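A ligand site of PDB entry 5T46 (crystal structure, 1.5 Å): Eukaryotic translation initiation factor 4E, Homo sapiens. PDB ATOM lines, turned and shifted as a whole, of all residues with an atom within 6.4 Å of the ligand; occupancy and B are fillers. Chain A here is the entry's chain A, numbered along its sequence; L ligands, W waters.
O of Lys 165 sits at hydrogen-bond distance from N of Asn 158, 2.8 Å away.
The guanidinium group (NH2) of Arg 160 lies within salt-bridge range of the side-chain carboxylate (OD1) of Asp 93 (2.9 Å).
The backbone carbonyl oxygen (O) of Gly 91 lies close to the guanidinium group (NH1) of Arg 160, at 3.4 Å.
Water W7 lies within hydrogen-bond range of O8 of the ligand (2.6 Å), NH2 of Arg 115 (2.9 Å) and NZ of Lys 165 (3.1 Å).
Water W9 lies within hydrogen-bond range of an oxygen (O2) of the ligand (2.7 Å), the side-chain amide oxygen (OD1) of Asn 158 (2.7 Å), the guanidinium group (NH1) of Arg 115 (2.9 Å) and the side-chain amino group (NZ) of Lys 165 (3.2 Å).
Water W6 lies within hydrogen-bond range of the side-chain carboxylate of Asp 93 (2.8 Å), an oxygen (O1) of the ligand (2.8 Å), the indole nitrogen of Trp 59 (2.9 Å) and the guanidinium group of Arg 160 (3.4 Å).
Water W2 lies within hydrogen-bond range of OE1 of Gln 60 (2.6 Å) and N4 of the ligand (3.3 Å).
The indole nitrogen of Trp 59 sits close to a nitrogen (N1) of the ligand.
Merely in contact with the ligand: Met 104 (3.1 Å).
Hydrophobic or aromatic side chains that line the ligand: Trp 59, Met 104 and Trp 105.
Seven residues have an atom within 4 Å of the ligand: Trp 59, Met 104, Trp 105, Glu 106, Arg 160, Lys 165 and Lys 209.
The nearest printed residue that does not touch the ligand is Trp 169 (4.2 Å).
The side-chain carboxylate of Glu 106 lies within hydrogen-bond range of a nitrogen (N4) of the ligand (2.6 Å).
The side-chain amino group of Lys 165 lies within salt-bridge range of an oxygen (O6) of the ligand, 2.7 Å away.
The backbone NH of Trp 105 is in hydrogen-bond range of an oxygen (O14) of the ligand (2.8 Å).
NH2 of Arg 160 lies within salt-bridge range of O1 of the ligand (2.8 Å).
NZ of Lys 209 is in salt-bridge range of O9 of the ligand (3.3 Å).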
ATOM      1  N   PHE A  51      24.500   6.540  11.715  1.00  0.00           N
ATOM      2  CA  PHE A  51      25.168   5.246  11.568  1.00  0.00           C
ATOM      3  C   PHE A  51      25.959   5.261  10.274  1.00  0.00           C
ATOM      4  O   PHE A  51      25.397   5.573   9.214  1.00  0.00           O
ATOM      5  CB  PHE A  51      24.163   4.079  11.553  1.00  0.00           C
ATOM      6  CG  PHE A  51      24.811   2.723  11.380  1.00  0.00           C
ATOM      7  CD1 PHE A  51      25.021   2.197  10.121  1.00  0.00           C
ATOM      8  CD2 PHE A  51      25.165   1.953  12.488  1.00  0.00           C
ATOM      9  CE1 PHE A  51      25.614   0.952   9.955  1.00  0.00           C
ATOM     10  CE2 PHE A  51      25.751   0.721  12.339  1.00  0.00           C
ATOM     11  CZ  PHE A  51      25.973   0.218  11.062  1.00  0.00           C
ATOM     12  N   LYS A  55      31.825  -2.262   7.645  1.00  0.00           N
ATOM     13  CA  LYS A  55      31.660  -3.656   8.024  1.00  0.00           C
ATOM     14  C   LYS A  55      32.853  -4.193   8.802  1.00  0.00           C
ATOM     15  O   LYS A  55      32.773  -5.311   9.323  1.00  0.00           O
ATOM     16  CB  LYS A  55      31.394  -4.526   6.792  1.00  0.00           C
ATOM     17  CG  LYS A  55      30.049  -4.235   6.098  1.00  0.00           C
ATOM     18  CD  LYS A  55      28.852  -4.603   6.965  1.00  0.00           C
ATOM     19  CE  LYS A  55      27.531  -4.471   6.222  1.00  0.00           C
ATOM     20  NZ  LYS A  55      27.012  -3.063   6.159  1.00  0.00           N
ATOM     21  N   TRP A  59      28.707  -3.584  15.042  1.00  0.00           N
ATOM     22  CA  TRP A  59      27.629  -2.695  14.606  1.00  0.00           C
ATOM     23  C   TRP A  59      27.535  -1.428  15.453  1.00  0.00           C
ATOM     24  O   TRP A  59      27.547  -0.323  14.904  1.00  0.00           O
ATOM     25  CB  TRP A  59      26.301  -3.482  14.575  1.00  0.00           C
ATOM     26  CG  TRP A  59      25.133  -2.680  14.121  1.00  0.00           C
ATOM     27  CD1 TRP A  59      24.710  -2.473  12.843  1.00  0.00           C
ATOM     28  CD2 TRP A  59      24.240  -1.950  14.965  1.00  0.00           C
ATOM     29  NE1 TRP A  59      23.604  -1.629  12.841  1.00  0.00           N
ATOM     30  CE2 TRP A  59      23.311  -1.301  14.142  1.00  0.00           C
ATOM     31  CE3 TRP A  59      24.162  -1.763  16.344  1.00  0.00           C
ATOM     32  CZ2 TRP A  59      22.313  -0.489  14.653  1.00  0.00           C
ATOM     33  CZ3 TRP A  59      23.176  -0.979  16.846  1.00  0.00           C
ATOM     34  CH2 TRP A  59      22.255  -0.342  16.004  1.00  0.00           C
ATOM     35  N   GLN A  60      27.491  -1.541  16.778  1.00  0.00           N
ATOM     36  CA  GLN A  60      27.290  -0.338  17.595  1.00  0.00           C
ATOM     37  C   GLN A  60      28.478   0.608  17.536  1.00  0.00           C
ATOM     38  O   GLN A  60      28.326   1.789  17.865  1.00  0.00           O
ATOM     39  CB  GLN A  60      26.992  -0.649  19.062  1.00  0.00           C
ATOM     40  CG  GLN A  60      28.070  -1.379  19.807  1.00  0.00           C
ATOM     41  CD  GLN A  60      27.813  -2.836  19.812  1.00  0.00           C
ATOM     42  OE1 GLN A  60      27.224  -3.366  18.872  1.00  0.00           O
ATOM     43  NE2 GLN A  60      28.218  -3.508  20.869  1.00  0.00           N
ATOM     44  N   GLY A  91      23.913   2.546   3.008  1.00  0.00           N
ATOM     45  CA  GLY A  91      24.430   1.862   4.170  1.00  0.00           C
ATOM     46  C   GLY A  91      24.384   2.691   5.436  1.00  0.00           C
ATOM     47  O   GLY A  91      24.629   2.139   6.522  1.00  0.00           O
ATOM     48  N   ASP A  93      22.428   5.369   8.282  1.00  0.00           N
ATOM     49  CA  ASP A  93      21.153   5.569   8.948  1.00  0.00           C
ATOM     50  C   ASP A  93      21.153   6.883   9.700  1.00  0.00           C
ATOM     51  O   ASP A  93      22.196   7.346  10.172  1.00  0.00           O
ATOM     52  CB  ASP A  93      20.834   4.521  10.048  1.00  0.00           C
ATOM     53  CG  ASP A  93      21.037   3.093   9.635  1.00  0.00           C
ATOM     54  OD1 ASP A  93      20.852   2.739   8.453  1.00  0.00           O
ATOM     55  OD2 ASP A  93      21.313   2.279  10.563  1.00  0.00           O
ATOM     56  N   PRO A 103      19.749   3.418  20.377  1.00  0.00           N
ATOM     57  CA  PRO A 103      18.999   3.062  19.158  1.00  0.00           C
ATOM     58  C   PRO A 103      19.314   1.657  18.685  1.00  0.00           C
ATOM     59  O   PRO A 103      19.741   1.441  17.543  1.00  0.00           O
ATOM     60  CB  PRO A 103      19.464   4.127  18.168  1.00  0.00           C
ATOM     61  CG  PRO A 103      20.874   4.388  18.567  1.00  0.00           C
ATOM     62  CD  PRO A 103      20.891   4.305  20.069  1.00  0.00           C
ATOM     63  N   MET A 104      19.116   0.695  19.580  1.00  0.00           N
ATOM     64  CA  MET A 104      19.452  -0.689  19.285  1.00  0.00           C
ATOM     65  C   MET A 104      18.518  -1.615  20.053  1.00  0.00           C
ATOM     66  O   MET A 104      17.951  -1.246  21.093  1.00  0.00           O
ATOM     67  CB  MET A 104      20.921  -0.975  19.623  1.00  0.00           C
ATOM     68  CG  MET A 104      21.386  -0.578  20.995  1.00  0.00           C
ATOM     69  SD  MET A 104      23.204  -0.520  21.019  1.00  0.00           S
ATOM     70  CE  MET A 104      23.641  -2.160  20.428  1.00  0.00           C
ATOM     71  N   TRP A 105      18.356  -2.825  19.509  1.00  0.00           N
ATOM     72  CA  TRP A 105      17.433  -3.816  20.050  1.00  0.00           C
ATOM     73  C   TRP A 105      17.689  -4.095  21.516  1.00  0.00           C
ATOM     74  O   TRP A 105      16.748  -4.382  22.280  1.00  0.00           O
ATOM     75  CB  TRP A 105      17.577  -5.141  19.311  1.00  0.00           C
ATOM     76  CG  TRP A 105      17.402  -5.097  17.873  1.00  0.00           C
ATOM     77  CD1 TRP A 105      16.529  -4.335  17.163  1.00  0.00           C
ATOM     78  CD2 TRP A 105      18.127  -5.888  16.931  1.00  0.00           C
ATOM     79  NE1 TRP A 105      16.666  -4.607  15.813  1.00  0.00           N
ATOM     80  CE2 TRP A 105      17.631  -5.562  15.648  1.00  0.00           C
ATOM     81  CE3 TRP A 105      19.134  -6.845  17.050  1.00  0.00           C
ATOM     82  CZ2 TRP A 105      18.128  -6.152  14.497  1.00  0.00           C
ATOM     83  CZ3 TRP A 105      19.618  -7.421  15.908  1.00  0.00           C
ATOM     84  CH2 TRP A 105      19.121  -7.075  14.640  1.00  0.00           C
ATOM     85  N   GLU A 106      18.968  -4.071  21.902  1.00  0.00           N
ATOM     86  CA  GLU A 106      19.408  -4.508  23.226  1.00  0.00           C
ATOM     87  C   GLU A 106      18.966  -3.588  24.350  1.00  0.00           C
ATOM     88  O   GLU A 106      18.943  -4.013  25.510  1.00  0.00           O
ATOM     89  CB  GLU A 106      20.918  -4.594  23.238  1.00  0.00           C
ATOM     90  CG  GLU A 106      21.471  -5.749  22.410  1.00  0.00           C
ATOM     91  CD  GLU A 106      21.819  -5.411  20.972  1.00  0.00           C
ATOM     92  OE1 GLU A 106      21.260  -4.463  20.380  1.00  0.00           O
ATOM     93  OE2 GLU A 106      22.711  -6.125  20.440  1.00  0.00           O
ATOM     94  N   ARG A 115       8.847  -2.661  15.613  1.00  0.00           N
ATOM     95  CA  ARG A 115       8.824  -1.495  14.744  1.00  0.00           C
ATOM     96  C   ARG A 115       7.681  -1.569  13.739  1.00  0.00           C
ATOM     97  O   ARG A 115       7.334  -2.646  13.241  1.00  0.00           O
ATOM     98  CB  ARG A 115      10.162  -1.367  13.997  1.00  0.00           C
ATOM     99  CG  ARG A 115      10.436  -2.460  13.008  1.00  0.00           C
ATOM    100  CD  ARG A 115      11.753  -2.236  12.293  1.00  0.00           C
ATOM    101  NE  ARG A 115      12.064  -3.376  11.445  1.00  0.00           N
ATOM    102  CZ  ARG A 115      13.126  -3.436  10.639  1.00  0.00           C
ATOM    103  NH1 ARG A 115      13.971  -2.419  10.605  1.00  0.00           N
ATOM    104  NH2 ARG A 115      13.338  -4.510   9.895  1.00  0.00           N
ATOM    105  N   ASN A 158      16.804   3.961   7.287  1.00  0.00           N
ATOM    106  CA  ASN A 158      17.903   3.217   6.678  1.00  0.00           C
ATOM    107  C   ASN A 158      17.986   3.579   5.199  1.00  0.00           C
ATOM    108  O   ASN A 158      17.047   3.313   4.445  1.00  0.00           O
ATOM    109  CB  ASN A 158      17.689   1.712   6.771  1.00  0.00           C
ATOM    110  CG  ASN A 158      17.382   1.221   8.174  1.00  0.00           C
ATOM    111  OD1 ASN A 158      16.314   0.669   8.406  1.00  0.00           O
ATOM    112  ND2 ASN A 158      18.336   1.346   9.089  1.00  0.00           N
ATOM    113  N   ARG A 160      19.337   2.486   1.844  1.00  0.00           N
ATOM    114  CA  ARG A 160      19.817   1.195   1.341  1.00  0.00           C
ATOM    115  C   ARG A 160      19.592   1.057  -0.147  1.00  0.00           C
ATOM    116  O   ARG A 160      18.543   1.450  -0.669  1.00  0.00           O
ATOM    117  CB  ARG A 160      19.101   0.026   2.047  1.00  0.00           C
ATOM    118  CG  ARG A 160      19.310  -0.036   3.534  1.00  0.00           C
ATOM    119  CD  ARG A 160      20.730  -0.421   3.862  1.00  0.00           C
ATOM    120  NE  ARG A 160      20.892  -0.601   5.300  1.00  0.00           N
ATOM    121  CZ  ARG A 160      21.152   0.371   6.171  1.00  0.00           C
ATOM    122  NH1 ARG A 160      21.310   1.625   5.764  1.00  0.00           N
ATOM    123  NH2 ARG A 160      21.271   0.082   7.463  1.00  0.00           N
ATOM    124  N   GLY A 163      16.439  -0.721  -1.093  1.00  0.00           N
ATOM    125  CA  GLY A 163      15.187  -0.103  -0.738  1.00  0.00           C
ATOM    126  C   GLY A 163      15.298   0.575   0.607  1.00  0.00           C
ATOM    127  O   GLY A 163      15.630  -0.066   1.606  1.00  0.00           O
ATOM    128  N   LYS A 165      14.292   2.276   4.134  1.00  0.00           N
ATOM    129  CA  LYS A 165      13.320   1.895   5.152  1.00  0.00           C
ATOM    130  C   LYS A 165      13.155   3.020   6.156  1.00  0.00           C
ATOM    131  O   LYS A 165      14.109   3.718   6.497  1.00  0.00           O
ATOM    132  CB  LYS A 165      13.740   0.628   5.863  1.00  0.00           C
ATOM    133  CG  LYS A 165      13.650  -0.599   4.972  1.00  0.00           C
ATOM    134  CD  LYS A 165      14.191  -1.824   5.654  1.00  0.00           C
ATOM    135  CE  LYS A 165      15.717  -1.831   5.661  1.00  0.00           C
ATOM    136  NZ  LYS A 165      16.245  -3.141   6.155  1.00  0.00           N
ATOM    137  N   TRP A 169       9.938   2.759  16.256  1.00  0.00           N
ATOM    138  CA  TRP A 169      10.178   1.725  17.255  1.00  0.00           C
ATOM    139  C   TRP A 169       9.346   1.969  18.495  1.00  0.00           C
ATOM    140  O   TRP A 169       9.332   3.103  19.018  1.00  0.00           O
ATOM    141  CB  TRP A 169      11.648   1.726  17.646  1.00  0.00           C
ATOM    142  CG  TRP A 169      12.595   1.191  16.611  1.00  0.00           C
ATOM    143  CD1 TRP A 169      12.458   1.224  15.243  1.00  0.00           C
ATOM    144  CD2 TRP A 169      13.830   0.521  16.874  1.00  0.00           C
ATOM    145  NE1 TRP A 169      13.558   0.607  14.653  1.00  0.00           N
ATOM    146  CE2 TRP A 169      14.404   0.182  15.641  1.00  0.00           C
ATOM    147  CE3 TRP A 169      14.504   0.189  18.052  1.00  0.00           C
ATOM    148  CZ2 TRP A 169      15.641  -0.486  15.544  1.00  0.00           C
ATOM    149  CZ3 TRP A 169      15.717  -0.468  17.972  1.00  0.00           C
ATOM    150  CH2 TRP A 169      16.274  -0.813  16.725  1.00  0.00           C
ATOM    151  N   THR A 206      12.970  -9.830  14.085  1.00  0.00           N
ATOM    152  CA  THR A 206      13.978  -9.275  13.198  1.00  0.00           C
ATOM    153  C   THR A 206      15.338  -9.892  13.467  1.00  0.00           C
ATOM    154  O   THR A 206      16.035 -10.309  12.543  1.00  0.00           O
ATOM    155  CB  THR A 206      14.054  -7.759  13.351  1.00  0.00           C
ATOM    156  OG1 THR A 206      12.748  -7.208  13.210  1.00  0.00           O
ATOM    157  CG2 THR A 206      14.980  -7.149  12.293  1.00  0.00           C
ATOM    158  N   ALA A 207      15.745  -9.929  14.742  1.00  0.00           N
ATOM    159  CA  ALA A 207      17.093 -10.416  15.074  1.00  0.00           C
ATOM    160  C   ALA A 207      17.292 -11.848  14.615  1.00  0.00           C
ATOM    161  O   ALA A 207      18.390 -12.223  14.185  1.00  0.00           O
ATOM    162  CB  ALA A 207      17.335 -10.286  16.575  1.00  0.00           C
ATOM    163  N   LYS A 209      15.609 -13.143  12.129  1.00  0.00           N
ATOM    164  CA  LYS A 209      15.303 -13.190  10.711  1.00  0.00           C
ATOM    165  C   LYS A 209      14.223 -14.231  10.430  1.00  0.00           C
ATOM    166  O   LYS A 209      13.181 -14.264  11.086  1.00  0.00           O
ATOM    167  CB  LYS A 209      16.558 -13.491   9.896  1.00  0.00           C
ATOM    168  CG  LYS A 209      17.571 -12.358   9.904  1.00  0.00           C
ATOM    169  CD  LYS A 209      18.934 -12.818   9.403  1.00  0.00           C
ATOM    170  CE  LYS A 209      19.833 -11.650   9.044  1.00  0.00           C
ATOM    171  NZ  LYS A 209      19.332 -10.913   7.850  1.00  0.00           N
HETATM  172  P1  LIG L   1      19.937  -3.289   9.200  1.00  0.00           P
HETATM  173  O1  LIG L   1      20.967  -2.265   8.986  1.00  0.00           O
HETATM  174  O2  LIG L   1      18.765  -2.809  10.116  1.00  0.00           O
HETATM  175  O3  LIG L   1      19.260  -3.772   7.842  1.00  0.00           O
HETATM  176  O4  LIG L   1      20.610  -4.542   9.926  1.00  0.00           O
HETATM  177  P2  LIG L   1      19.811  -4.007   6.379  1.00  0.00           P
HETATM  178  O5  LIG L   1      21.190  -3.477   6.180  1.00  0.00           O
HETATM  179  O6  LIG L   1      18.831  -3.345   5.374  1.00  0.00           O
HETATM  180  O7  LIG L   1      19.775  -5.562   6.113  1.00  0.00           O
HETATM  181  P3  LIG L   1      18.729  -6.735   6.388  1.00  0.00           P
HETATM  182  O8  LIG L   1      17.377  -6.271   6.763  1.00  0.00           O
HETATM  183  O9  LIG L   1      19.315  -7.602   7.554  1.00  0.00           O
HETATM  184  O10 LIG L   1      18.627  -7.535   5.053  1.00  0.00           O
HETATM  185  C1  LIG L   1      21.681  -5.219   9.363  1.00  0.00           C
HETATM  186  C2  LIG L   1      22.464  -5.866  10.522  1.00  0.00           C
HETATM  187  O11 LIG L   1      22.895  -4.841  11.417  1.00  0.00           O
HETATM  188  C3  LIG L   1      21.643  -6.847  11.392  1.00  0.00           C
HETATM  189  O12 LIG L   1      21.622  -8.090  10.801  1.00  0.00           O
HETATM  190  C4  LIG L   1      22.565  -6.872  12.642  1.00  0.00           C
HETATM  191  O13 LIG L   1      23.701  -7.623  12.390  1.00  0.00           O
HETATM  192  C5  LIG L   1      23.004  -5.378  12.699  1.00  0.00           C
HETATM  193  N1  LIG L   1      22.036  -4.642  13.522  1.00  0.00           N
HETATM  194  C6  LIG L   1      21.011  -3.808  13.083  1.00  0.00           C
HETATM  195  N2  LIG L   1      20.375  -3.324  14.175  1.00  0.00           N
HETATM  196  C7  LIG L   1      19.227  -2.432  14.179  1.00  0.00           C
HETATM  197  C8  LIG L   1      21.004  -3.839  15.311  1.00  0.00           C
HETATM  198  C9  LIG L   1      20.718  -3.653  16.693  1.00  0.00           C
HETATM  199  O14 LIG L   1      19.863  -2.948  17.177  1.00  0.00           O
HETATM  200  N3  LIG L   1      21.586  -4.419  17.538  1.00  0.00           N
HETATM  201  C10 LIG L   1      22.607  -5.209  17.025  1.00  0.00           C
HETATM  202  N4  LIG L   1      23.399  -5.833  17.915  1.00  0.00           N
HETATM  203  N5  LIG L   1      22.897  -5.392  15.687  1.00  0.00           N
HETATM  204  C11 LIG L   1      22.046  -4.671  14.889  1.00  0.00           C
HETATM  205  O   HOH W   1      19.169   0.590  12.828  1.00  0.00           O
HETATM  206  O   HOH W   2      26.697  -5.790  17.940  1.00  0.00           O
HETATM  207  O   HOH W   3      17.302  -4.853  11.051  1.00  0.00           O
HETATM  208  O   HOH W   4      23.837  -2.005   8.886  1.00  0.00           O
HETATM  209  O   HOH W   5      16.895  -0.863  12.082  1.00  0.00           O
HETATM  210  O   HOH W   6      22.066  -0.391  10.778  1.00  0.00           O
HETATM  211  O   HOH W   7      15.915  -5.083   8.606  1.00  0.00           O
HETATM  212  O   HOH W   8      18.639  -3.599   2.840  1.00  0.00           O
HETATM  213  O   HOH W   9      16.382  -1.970   9.094  1.00  0.00           O
